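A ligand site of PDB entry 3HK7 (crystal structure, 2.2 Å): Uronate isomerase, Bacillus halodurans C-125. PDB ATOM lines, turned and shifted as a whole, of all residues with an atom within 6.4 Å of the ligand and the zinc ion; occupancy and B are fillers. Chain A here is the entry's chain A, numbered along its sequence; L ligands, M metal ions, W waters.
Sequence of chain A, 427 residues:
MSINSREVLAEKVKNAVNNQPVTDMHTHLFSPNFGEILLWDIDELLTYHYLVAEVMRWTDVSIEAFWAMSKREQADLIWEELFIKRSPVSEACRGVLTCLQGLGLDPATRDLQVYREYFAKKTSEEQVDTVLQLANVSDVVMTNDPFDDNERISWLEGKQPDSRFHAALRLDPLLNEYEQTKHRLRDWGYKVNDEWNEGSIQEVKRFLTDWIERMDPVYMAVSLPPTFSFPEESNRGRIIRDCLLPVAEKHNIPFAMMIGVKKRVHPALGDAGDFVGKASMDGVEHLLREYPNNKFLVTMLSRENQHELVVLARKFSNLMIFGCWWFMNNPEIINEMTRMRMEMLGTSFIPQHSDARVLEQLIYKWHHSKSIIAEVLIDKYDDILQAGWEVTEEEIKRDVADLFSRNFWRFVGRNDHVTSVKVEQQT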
ATOM      1  N   HIS A  26     -32.944  21.242  -4.453  1.00  0.00           N
ATOM      2  CA  HIS A  26     -31.935  20.205  -4.676  1.00  0.00           C
ATOM      3  C   HIS A  26     -31.128  19.909  -3.422  1.00  0.00           C
ATOM      4  O   HIS A  26     -30.341  20.744  -2.962  1.00  0.00           O
ATOM      5  CB  HIS A  26     -30.956  20.544  -5.809  1.00  0.00           C
ATOM      6  CG  HIS A  26     -29.906  19.483  -6.014  1.00  0.00           C
ATOM      7  ND1 HIS A  26     -30.220  18.193  -6.383  1.00  0.00           N
ATOM      8  CD2 HIS A  26     -28.563  19.509  -5.834  1.00  0.00           C
ATOM      9  CE1 HIS A  26     -29.118  17.466  -6.427  1.00  0.00           C
ATOM     10  NE2 HIS A  26     -28.091  18.241  -6.101  1.00  0.00           N
ATOM     11  N   THR A  27     -31.331  18.718  -2.877  1.00  0.00           N
ATOM     12  CA  THR A  27     -30.624  18.284  -1.673  1.00  0.00           C
ATOM     13  C   THR A  27     -30.418  16.787  -1.753  1.00  0.00           C
ATOM     14  O   THR A  27     -30.948  16.126  -2.655  1.00  0.00           O
ATOM     15  CB  THR A  27     -31.429  18.550  -0.376  1.00  0.00           C
ATOM     16  OG1 THR A  27     -32.496  17.591  -0.282  1.00  0.00           O
ATOM     17  CG2 THR A  27     -32.027  19.949  -0.385  1.00  0.00           C
ATOM     18  N   HIS A  28     -29.655  16.269  -0.803  1.00  0.00           N
ATOM     19  CA  HIS A  28     -29.392  14.842  -0.700  1.00  0.00           C
ATOM     20  C   HIS A  28     -29.923  14.389   0.647  1.00  0.00           C
ATOM     21  O   HIS A  28     -29.338  13.541   1.319  1.00  0.00           O
ATOM     22  CB  HIS A  28     -27.896  14.605  -0.820  1.00  0.00           C
ATOM     23  CG  HIS A  28     -27.382  14.801  -2.211  1.00  0.00           C
ATOM     24  ND1 HIS A  28     -27.533  13.845  -3.190  1.00  0.00           N
ATOM     25  CD2 HIS A  28     -26.823  15.878  -2.813  1.00  0.00           C
ATOM     26  CE1 HIS A  28     -27.085  14.331  -4.339  1.00  0.00           C
ATOM     27  NE2 HIS A  28     -26.659  15.561  -4.137  1.00  0.00           N
ATOM     28  N   TYR A  48     -18.618  15.305   6.411  1.00  0.00           N
ATOM     29  CA  TYR A  48     -19.167  15.718   5.113  1.00  0.00           C
ATOM     30  C   TYR A  48     -17.960  15.563   4.185  1.00  0.00           C
ATOM     31  O   TYR A  48     -16.845  15.918   4.573  1.00  0.00           O
ATOM     32  CB  TYR A  48     -19.610  17.194   5.237  1.00  0.00           C
ATOM     33  CG  TYR A  48     -20.180  17.879   4.016  1.00  0.00           C
ATOM     34  CD1 TYR A  48     -21.027  17.224   3.128  1.00  0.00           C
ATOM     35  CD2 TYR A  48     -19.942  19.239   3.806  1.00  0.00           C
ATOM     36  CE1 TYR A  48     -21.651  17.911   2.070  1.00  0.00           C
ATOM     37  CE2 TYR A  48     -20.550  19.942   2.766  1.00  0.00           C
ATOM     38  CZ  TYR A  48     -21.400  19.271   1.905  1.00  0.00           C
ATOM     39  OH  TYR A  48     -22.015  19.986   0.908  1.00  0.00           O
ATOM     40  N   HIS A  49     -18.144  15.017   2.987  1.00  0.00           N
ATOM     41  CA  HIS A  49     -16.973  14.812   2.137  1.00  0.00           C
ATOM     42  C   HIS A  49     -16.183  16.082   1.828  1.00  0.00           C
ATOM     43  O   HIS A  49     -14.981  16.023   1.569  1.00  0.00           O
ATOM     44  CB  HIS A  49     -17.335  14.020   0.873  1.00  0.00           C
ATOM     45  CG  HIS A  49     -18.049  14.797  -0.192  1.00  0.00           C
ATOM     46  ND1 HIS A  49     -17.395  15.638  -1.065  1.00  0.00           N
ATOM     47  CD2 HIS A  49     -19.347  14.805  -0.571  1.00  0.00           C
ATOM     48  CE1 HIS A  49     -18.255  16.121  -1.952  1.00  0.00           C
ATOM     49  NE2 HIS A  49     -19.440  15.626  -1.677  1.00  0.00           N
ATOM     50  N   TYR A  50     -16.837  17.245   1.885  1.00  0.00           N
ATOM     51  CA  TYR A  50     -16.145  18.501   1.633  1.00  0.00           C
ATOM     52  C   TYR A  50     -15.033  18.653   2.688  1.00  0.00           C
ATOM     53  O   TYR A  50     -13.941  19.125   2.371  1.00  0.00           O
ATOM     54  CB  TYR A  50     -17.105  19.697   1.749  1.00  0.00           C
ATOM     55  CG  TYR A  50     -18.059  19.916   0.586  1.00  0.00           C
ATOM     56  CD1 TYR A  50     -18.731  18.850  -0.007  1.00  0.00           C
ATOM     57  CD2 TYR A  50     -18.359  21.209   0.141  1.00  0.00           C
ATOM     58  CE1 TYR A  50     -19.700  19.076  -1.001  1.00  0.00           C
ATOM     59  CE2 TYR A  50     -19.320  21.442  -0.844  1.00  0.00           C
ATOM     60  CZ  TYR A  50     -19.985  20.369  -1.415  1.00  0.00           C
ATOM     61  OH  TYR A  50     -20.949  20.600  -2.372  1.00  0.00           O
ATOM     62  N   THR A 143     -32.914  13.708  -3.827  1.00  0.00           N
ATOM     63  CA  THR A 143     -32.314  13.152  -5.032  1.00  0.00           C
ATOM     64  C   THR A 143     -32.609  11.667  -4.887  1.00  0.00           C
ATOM     65  O   THR A 143     -32.025  10.991  -4.056  1.00  0.00           O
ATOM     66  CB  THR A 143     -30.788  13.364  -5.060  1.00  0.00           C
ATOM     67  OG1 THR A 143     -30.494  14.772  -5.066  1.00  0.00           O
ATOM     68  CG2 THR A 143     -30.183  12.717  -6.304  1.00  0.00           C
ATOM     69  N   ARG A 170     -33.262  10.906 -10.150  1.00  0.00           N
ATOM     70  CA  ARG A 170     -31.885  10.995 -10.612  1.00  0.00           C
ATOM     71  C   ARG A 170     -31.580   9.819 -11.555  1.00  0.00           C
ATOM     72  O   ARG A 170     -31.780   8.664 -11.194  1.00  0.00           O
ATOM     73  CB  ARG A 170     -30.949  10.972  -9.398  1.00  0.00           C
ATOM     74  CG  ARG A 170     -29.508  11.353  -9.672  1.00  0.00           C
ATOM     75  CD  ARG A 170     -29.403  12.755 -10.269  1.00  0.00           C
ATOM     76  NE  ARG A 170     -27.998  13.102 -10.478  1.00  0.00           N
ATOM     77  CZ  ARG A 170     -27.239  13.732  -9.589  1.00  0.00           C
ATOM     78  NH1 ARG A 170     -27.754  14.107  -8.418  1.00  0.00           N
ATOM     79  NH2 ARG A 170     -25.966  13.952  -9.852  1.00  0.00           N
ATOM     80  N   ASP A 172     -28.371   9.345 -13.438  1.00  0.00           N
ATOM     81  CA  ASP A 172     -26.969   9.221 -13.837  1.00  0.00           C
ATOM     82  C   ASP A 172     -26.544   7.860 -14.416  1.00  0.00           C
ATOM     83  O   ASP A 172     -25.898   7.803 -15.473  1.00  0.00           O
ATOM     84  CB  ASP A 172     -26.061   9.587 -12.656  1.00  0.00           C
ATOM     85  CG  ASP A 172     -26.144  11.081 -12.295  1.00  0.00           C
ATOM     86  OD1 ASP A 172     -27.181  11.701 -12.620  1.00  0.00           O
ATOM     87  OD2 ASP A 172     -25.195  11.616 -11.671  1.00  0.00           O
ATOM     88  N   SER A 223     -26.233  14.428 -13.509  1.00  0.00           N
ATOM     89  CA  SER A 223     -25.031  15.255 -13.449  1.00  0.00           C
ATOM     90  C   SER A 223     -24.239  14.850 -14.691  1.00  0.00           C
ATOM     91  O   SER A 223     -24.154  13.676 -15.027  1.00  0.00           O
ATOM     92  CB  SER A 223     -24.229  14.978 -12.174  1.00  0.00           C
ATOM     93  OG  SER A 223     -23.705  13.670 -12.142  1.00  0.00           O
ATOM     94  N   MET A 258     -27.095  19.057 -14.419  1.00  0.00           N
ATOM     95  CA  MET A 258     -26.058  19.614 -13.574  1.00  0.00           C
ATOM     96  C   MET A 258     -24.741  19.271 -14.275  1.00  0.00           C
ATOM     97  O   MET A 258     -24.177  18.176 -14.112  1.00  0.00           O
ATOM     98  CB  MET A 258     -26.151  18.996 -12.176  1.00  0.00           C
ATOM     99  CG  MET A 258     -27.573  19.083 -11.610  1.00  0.00           C
ATOM    100  SD  MET A 258     -27.644  19.043  -9.813  1.00  0.00           S
ATOM    101  CE  MET A 258     -27.424  17.306  -9.532  1.00  0.00           C
ATOM    102  N   VAL A 261     -19.134  18.259 -13.840  1.00  0.00           N
ATOM    103  CA  VAL A 261     -18.426  17.366 -12.932  1.00  0.00           C
ATOM    104  C   VAL A 261     -17.588  16.292 -13.631  1.00  0.00           C
ATOM    105  O   VAL A 261     -18.065  15.608 -14.527  1.00  0.00           O
ATOM    106  CB  VAL A 261     -19.412  16.696 -11.924  1.00  0.00           C
ATOM    107  CG1 VAL A 261     -20.467  15.898 -12.677  1.00  0.00           C
ATOM    108  CG2 VAL A 261     -18.651  15.800 -10.959  1.00  0.00           C
ATOM    109  N   LYS A 263     -16.022  12.994 -12.832  1.00  0.00           N
ATOM    110  CA  LYS A 263     -16.037  11.964 -11.809  1.00  0.00           C
ATOM    111  C   LYS A 263     -14.757  11.183 -11.567  1.00  0.00           C
ATOM    112  O   LYS A 263     -14.010  10.868 -12.488  1.00  0.00           O
ATOM    113  CB  LYS A 263     -17.179  10.975 -12.091  1.00  0.00           C
ATOM    114  CG  LYS A 263     -18.521  11.630 -12.370  1.00  0.00           C
ATOM    115  CD  LYS A 263     -19.558  11.328 -11.286  1.00  0.00           C
ATOM    116  CE  LYS A 263     -19.213  12.009  -9.966  1.00  0.00           C
ATOM    117  NZ  LYS A 263     -20.287  11.833  -8.937  1.00  0.00           N
ATOM    118  N   ASP A 271     -16.554  10.032  -2.448  1.00  0.00           N
ATOM    119  CA  ASP A 271     -17.404  11.159  -2.834  1.00  0.00           C
ATOM    120  C   ASP A 271     -16.637  12.469  -2.937  1.00  0.00           C
ATOM    121  O   ASP A 271     -17.095  13.409  -3.580  1.00  0.00           O
ATOM    122  CB  ASP A 271     -18.561  11.332  -1.841  1.00  0.00           C
ATOM    123  CG  ASP A 271     -19.549  10.202  -1.888  1.00  0.00           C
ATOM    124  OD1 ASP A 271     -19.713   9.604  -2.979  1.00  0.00           O
ATOM    125  OD2 ASP A 271     -20.184   9.912  -0.854  1.00  0.00           O
ATOM    126  N   ALA A 272     -15.474  12.529  -2.309  1.00  0.00           N
ATOM    127  CA  ALA A 272     -14.646  13.729  -2.338  1.00  0.00           C
ATOM    128  C   ALA A 272     -13.626  13.717  -3.484  1.00  0.00           C
ATOM    129  O   ALA A 272     -12.757  14.588  -3.547  1.00  0.00           O
ATOM    130  CB  ALA A 272     -13.906  13.856  -1.007  1.00  0.00           C
ATOM    131  N   ASP A 274     -14.240  14.018  -6.927  1.00  0.00           N
ATOM    132  CA  ASP A 274     -14.702  14.539  -8.207  1.00  0.00           C
ATOM    133  C   ASP A 274     -14.068  15.912  -8.497  1.00  0.00           C
ATOM    134  O   ASP A 274     -13.859  16.699  -7.583  1.00  0.00           O
ATOM    135  CB  ASP A 274     -16.227  14.672  -8.232  1.00  0.00           C
ATOM    136  CG  ASP A 274     -16.924  13.329  -8.164  1.00  0.00           C
ATOM    137  OD1 ASP A 274     -16.407  12.356  -8.759  1.00  0.00           O
ATOM    138  OD2 ASP A 274     -17.993  13.247  -7.522  1.00  0.00           O
ATOM    139  N   TRP A 325     -23.776  25.737  -7.451  1.00  0.00           N
ATOM    140  CA  TRP A 325     -23.437  24.356  -7.206  1.00  0.00           C
ATOM    141  C   TRP A 325     -22.030  23.954  -6.797  1.00  0.00           C
ATOM    142  O   TRP A 325     -21.042  24.374  -7.410  1.00  0.00           O
ATOM    143  CB  TRP A 325     -23.831  23.553  -8.453  1.00  0.00           C
ATOM    144  CG  TRP A 325     -23.701  22.062  -8.365  1.00  0.00           C
ATOM    145  CD1 TRP A 325     -23.984  21.277  -7.287  1.00  0.00           C
ATOM    146  CD2 TRP A 325     -23.358  21.165  -9.430  1.00  0.00           C
ATOM    147  NE1 TRP A 325     -23.853  19.951  -7.611  1.00  0.00           N
ATOM    148  CE2 TRP A 325     -23.470  19.851  -8.929  1.00  0.00           C
ATOM    149  CE3 TRP A 325     -22.972  21.344 -10.768  1.00  0.00           C
ATOM    150  CZ2 TRP A 325     -23.203  18.715  -9.710  1.00  0.00           C
ATOM    151  CZ3 TRP A 325     -22.706  20.222 -11.549  1.00  0.00           C
ATOM    152  CH2 TRP A 325     -22.824  18.921 -11.019  1.00  0.00           C
ATOM    153  N   TRP A 326     -21.956  23.167  -5.727  1.00  0.00           N
ATOM    154  CA  TRP A 326     -20.698  22.575  -5.263  1.00  0.00           C
ATOM    155  C   TRP A 326     -19.510  23.517  -5.121  1.00  0.00           C
ATOM    156  O   TRP A 326     -19.427  24.296  -4.174  1.00  0.00           O
ATOM    157  CB  TRP A 326     -20.362  21.475  -6.269  1.00  0.00           C
ATOM    158  CG  TRP A 326     -19.609  20.283  -5.792  1.00  0.00           C
ATOM    159  CD1 TRP A 326     -18.689  20.223  -4.796  1.00  0.00           C
ATOM    160  CD2 TRP A 326     -19.601  18.998  -6.431  1.00  0.00           C
ATOM    161  NE1 TRP A 326     -18.101  18.979  -4.767  1.00  0.00           N
ATOM    162  CE2 TRP A 326     -18.645  18.206  -5.762  1.00  0.00           C
ATOM    163  CE3 TRP A 326     -20.320  18.442  -7.504  1.00  0.00           C
ATOM    164  CZ2 TRP A 326     -18.376  16.883  -6.138  1.00  0.00           C
ATOM    165  CZ3 TRP A 326     -20.052  17.134  -7.879  1.00  0.00           C
ATOM    166  CH2 TRP A 326     -19.092  16.371  -7.194  1.00  0.00           C
ATOM    167  N   HIS A 353     -29.602  26.631  -3.876  1.00  0.00           N
ATOM    168  CA  HIS A 353     -30.060  25.335  -3.379  1.00  0.00           C
ATOM    169  C   HIS A 353     -28.947  24.920  -2.397  1.00  0.00           C
ATOM    170  O   HIS A 353     -27.803  25.349  -2.552  1.00  0.00           O
ATOM    171  CB  HIS A 353     -30.233  24.311  -4.509  1.00  0.00           C
ATOM    172  CG  HIS A 353     -28.947  23.817  -5.093  1.00  0.00           C
ATOM    173  ND1 HIS A 353     -28.339  24.426  -6.178  1.00  0.00           N
ATOM    174  CD2 HIS A 353     -28.174  22.747  -4.779  1.00  0.00           C
ATOM    175  CE1 HIS A 353     -27.244  23.759  -6.498  1.00  0.00           C
ATOM    176  NE2 HIS A 353     -27.122  22.744  -5.663  1.00  0.00           N
ATOM    177  N   ASP A 355     -27.923  21.577  -1.468  1.00  0.00           N
ATOM    178  CA  ASP A 355     -27.172  20.380  -1.828  1.00  0.00           C
ATOM    179  C   ASP A 355     -26.803  19.655  -0.522  1.00  0.00           C
ATOM    180  O   ASP A 355     -25.809  18.933  -0.459  1.00  0.00           O
ATOM    181  CB  ASP A 355     -25.896  20.754  -2.576  1.00  0.00           C
ATOM    182  CG  ASP A 355     -25.678  19.913  -3.805  1.00  0.00           C
ATOM    183  OD1 ASP A 355     -25.799  18.671  -3.717  1.00  0.00           O
ATOM    184  OD2 ASP A 355     -25.392  20.484  -4.879  1.00  0.00           O
ATOM    185  N   ARG A 357     -26.262  17.145   2.350  1.00  0.00           N
ATOM    186  CA  ARG A 357     -26.101  15.706   2.467  1.00  0.00           C
ATOM    187  C   ARG A 357     -26.423  15.345   3.919  1.00  0.00           C
ATOM    188  O   ARG A 357     -26.872  14.235   4.206  1.00  0.00           O
ATOM    189  CB  ARG A 357     -24.658  15.278   2.151  1.00  0.00           C
ATOM    190  CG  ARG A 357     -24.367  15.032   0.670  1.00  0.00           C
ATOM    191  CD  ARG A 357     -22.882  14.717   0.479  1.00  0.00           C
ATOM    192  NE  ARG A 357     -22.539  14.424  -0.904  1.00  0.00           N
ATOM    193  CZ  ARG A 357     -22.701  13.238  -1.497  1.00  0.00           C
ATOM    194  NH1 ARG A 357     -23.216  12.220  -0.815  1.00  0.00           N
ATOM    195  NH2 ARG A 357     -22.348  13.069  -2.758  1.00  0.00           N
HETATM  196  O1  LIG L   1     -24.135  15.173  -8.319  1.00  0.00           O
HETATM  197  C1  LIG L   1     -24.572  15.900  -7.383  1.00  0.00           C
HETATM  198  O2  LIG L   1     -25.777  16.102  -7.145  1.00  0.00           O
HETATM  199  C2  LIG L   1     -23.539  16.597  -6.474  1.00  0.00           C
HETATM  200  O3  LIG L   1     -24.203  17.663  -5.780  1.00  0.00           O
HETATM  201  C3  LIG L   1     -22.901  15.627  -5.444  1.00  0.00           C
HETATM  202  O4  LIG L   1     -23.897  15.214  -4.495  1.00  0.00           O
HETATM  203  C4  LIG L   1     -21.688  16.250  -4.671  1.00  0.00           C
HETATM  204  O5  LIG L   1     -20.880  15.231  -4.077  1.00  0.00           O
HETATM  205  C5  LIG L   1     -22.101  17.236  -3.539  1.00  0.00           C
HETATM  206  O6  LIG L   1     -21.957  16.866  -2.352  1.00  0.00           O
HETATM  207  O7  LIG L   1     -22.559  18.358  -3.893  1.00  0.00           O
HETATM  208 ZN    ZN M   1     -26.224  17.366  -5.353  1.00  0.00          ZN
HETATM  209  O   HOH W   1     -19.020  13.590  -5.166  1.00  0.00           O
HETATM  210  O   HOH W   2     -22.315  13.901  -9.686  1.00  0.00           O
HETATM  211  O   HOH W   3     -23.291  18.412  -0.539  1.00  0.00           O
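Within 4 Å of the zinc ion: His 26, His 28 and Asp 355.
An oxygen (O1) of the ligand lies within salt-bridge range of the guanidinium group (NH2) of Arg 170 (2.7 Å). NE2 of His 49 is in hydrogen-bond range of O5 of the ligand. O6 of the ligand is in salt-bridge range of NE of Arg 357, at 2.9 Å. The indole nitrogen (NE1) of Trp 325 lies close to an oxygen (O3) of the ligand (3.0 Å). The side-chain hydroxyl (OH) of Tyr 50 lies within hydrogen-bond range of an oxygen (O7) of the ligand.
Merely in contact with the ligand: Ser 223 (3.9 Å), Met 258 (3.1 Å) and Trp 326 (3.6 Å). Hydrophobic or aromatic side chains within 4 Å of the ligand: His 26, His 28, His 49, Tyr 50, Met 258, Trp 325 and Trp 326. 11 residues have an atom within 4 Å of the ligand: His 26, His 28, His 49, Tyr 50, Arg 170, Ser 223, Met 258, Trp 325, Trp 326, Asp 355 and Arg 357.
Water W2 lies within hydrogen-bond range of O1 of the ligand (2.6 Å), OG of Ser 223 (2.8 Å) and NZ of Lys 263 (3.0 Å). Water W1 lies within hydrogen-bond range of the backbone carbonyl oxygen (O) of Asp 271 (2.5 Å), the side-chain carboxylate (OD2) of Asp 274 (2.6 Å) and an oxygen (O5) of the ligand (2.7 Å). Water W3 lies within hydrogen-bond range of OH of Tyr 48, O of Asp 355 and O6 of the ligand.
The zinc ion is bound by an oxygen (O3) of the ligand (2.1 Å), the side-chain carboxylate of Asp 355 (2.1 Å), a ring nitrogen (NE2) of His 26 (2.2 Å), a ring nitrogen (NE2) of His 28 (2.2 Å) and an oxygen (O2) of the ligand (2.2 Å).
The indole nitrogen of Trp 325 lies close to the side-chain carboxylate of Asp 355. NE2 of His 353 is in hydrogen-bond range of OD2 of Asp 355 (3.0 Å). The side-chain hydroxyl (OG) of Ser 223 lies close to the guanidinium group (NH2) of Arg 170 (3.2 Å). OD1 of Asp 172 is in salt-bridge range of NE of Arg 170, 2.7 Å away. The guanidinium group (NE) of Arg 357 lies close to a ring nitrogen (NE2) of His 49, at 3.4 Å. ND1 of His 49 sits close to O of Asp 271 (3.4 Å). The guanidinium group of Arg 357 lies within salt-bridge range of the side-chain carboxylate of Asp 271 (3.8 Å). The side-chain carboxylate (OD2) of Asp 172 is in hydrogen-bond range of the side-chain hydroxyl (OG) of Ser 223 (2.6 Å).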
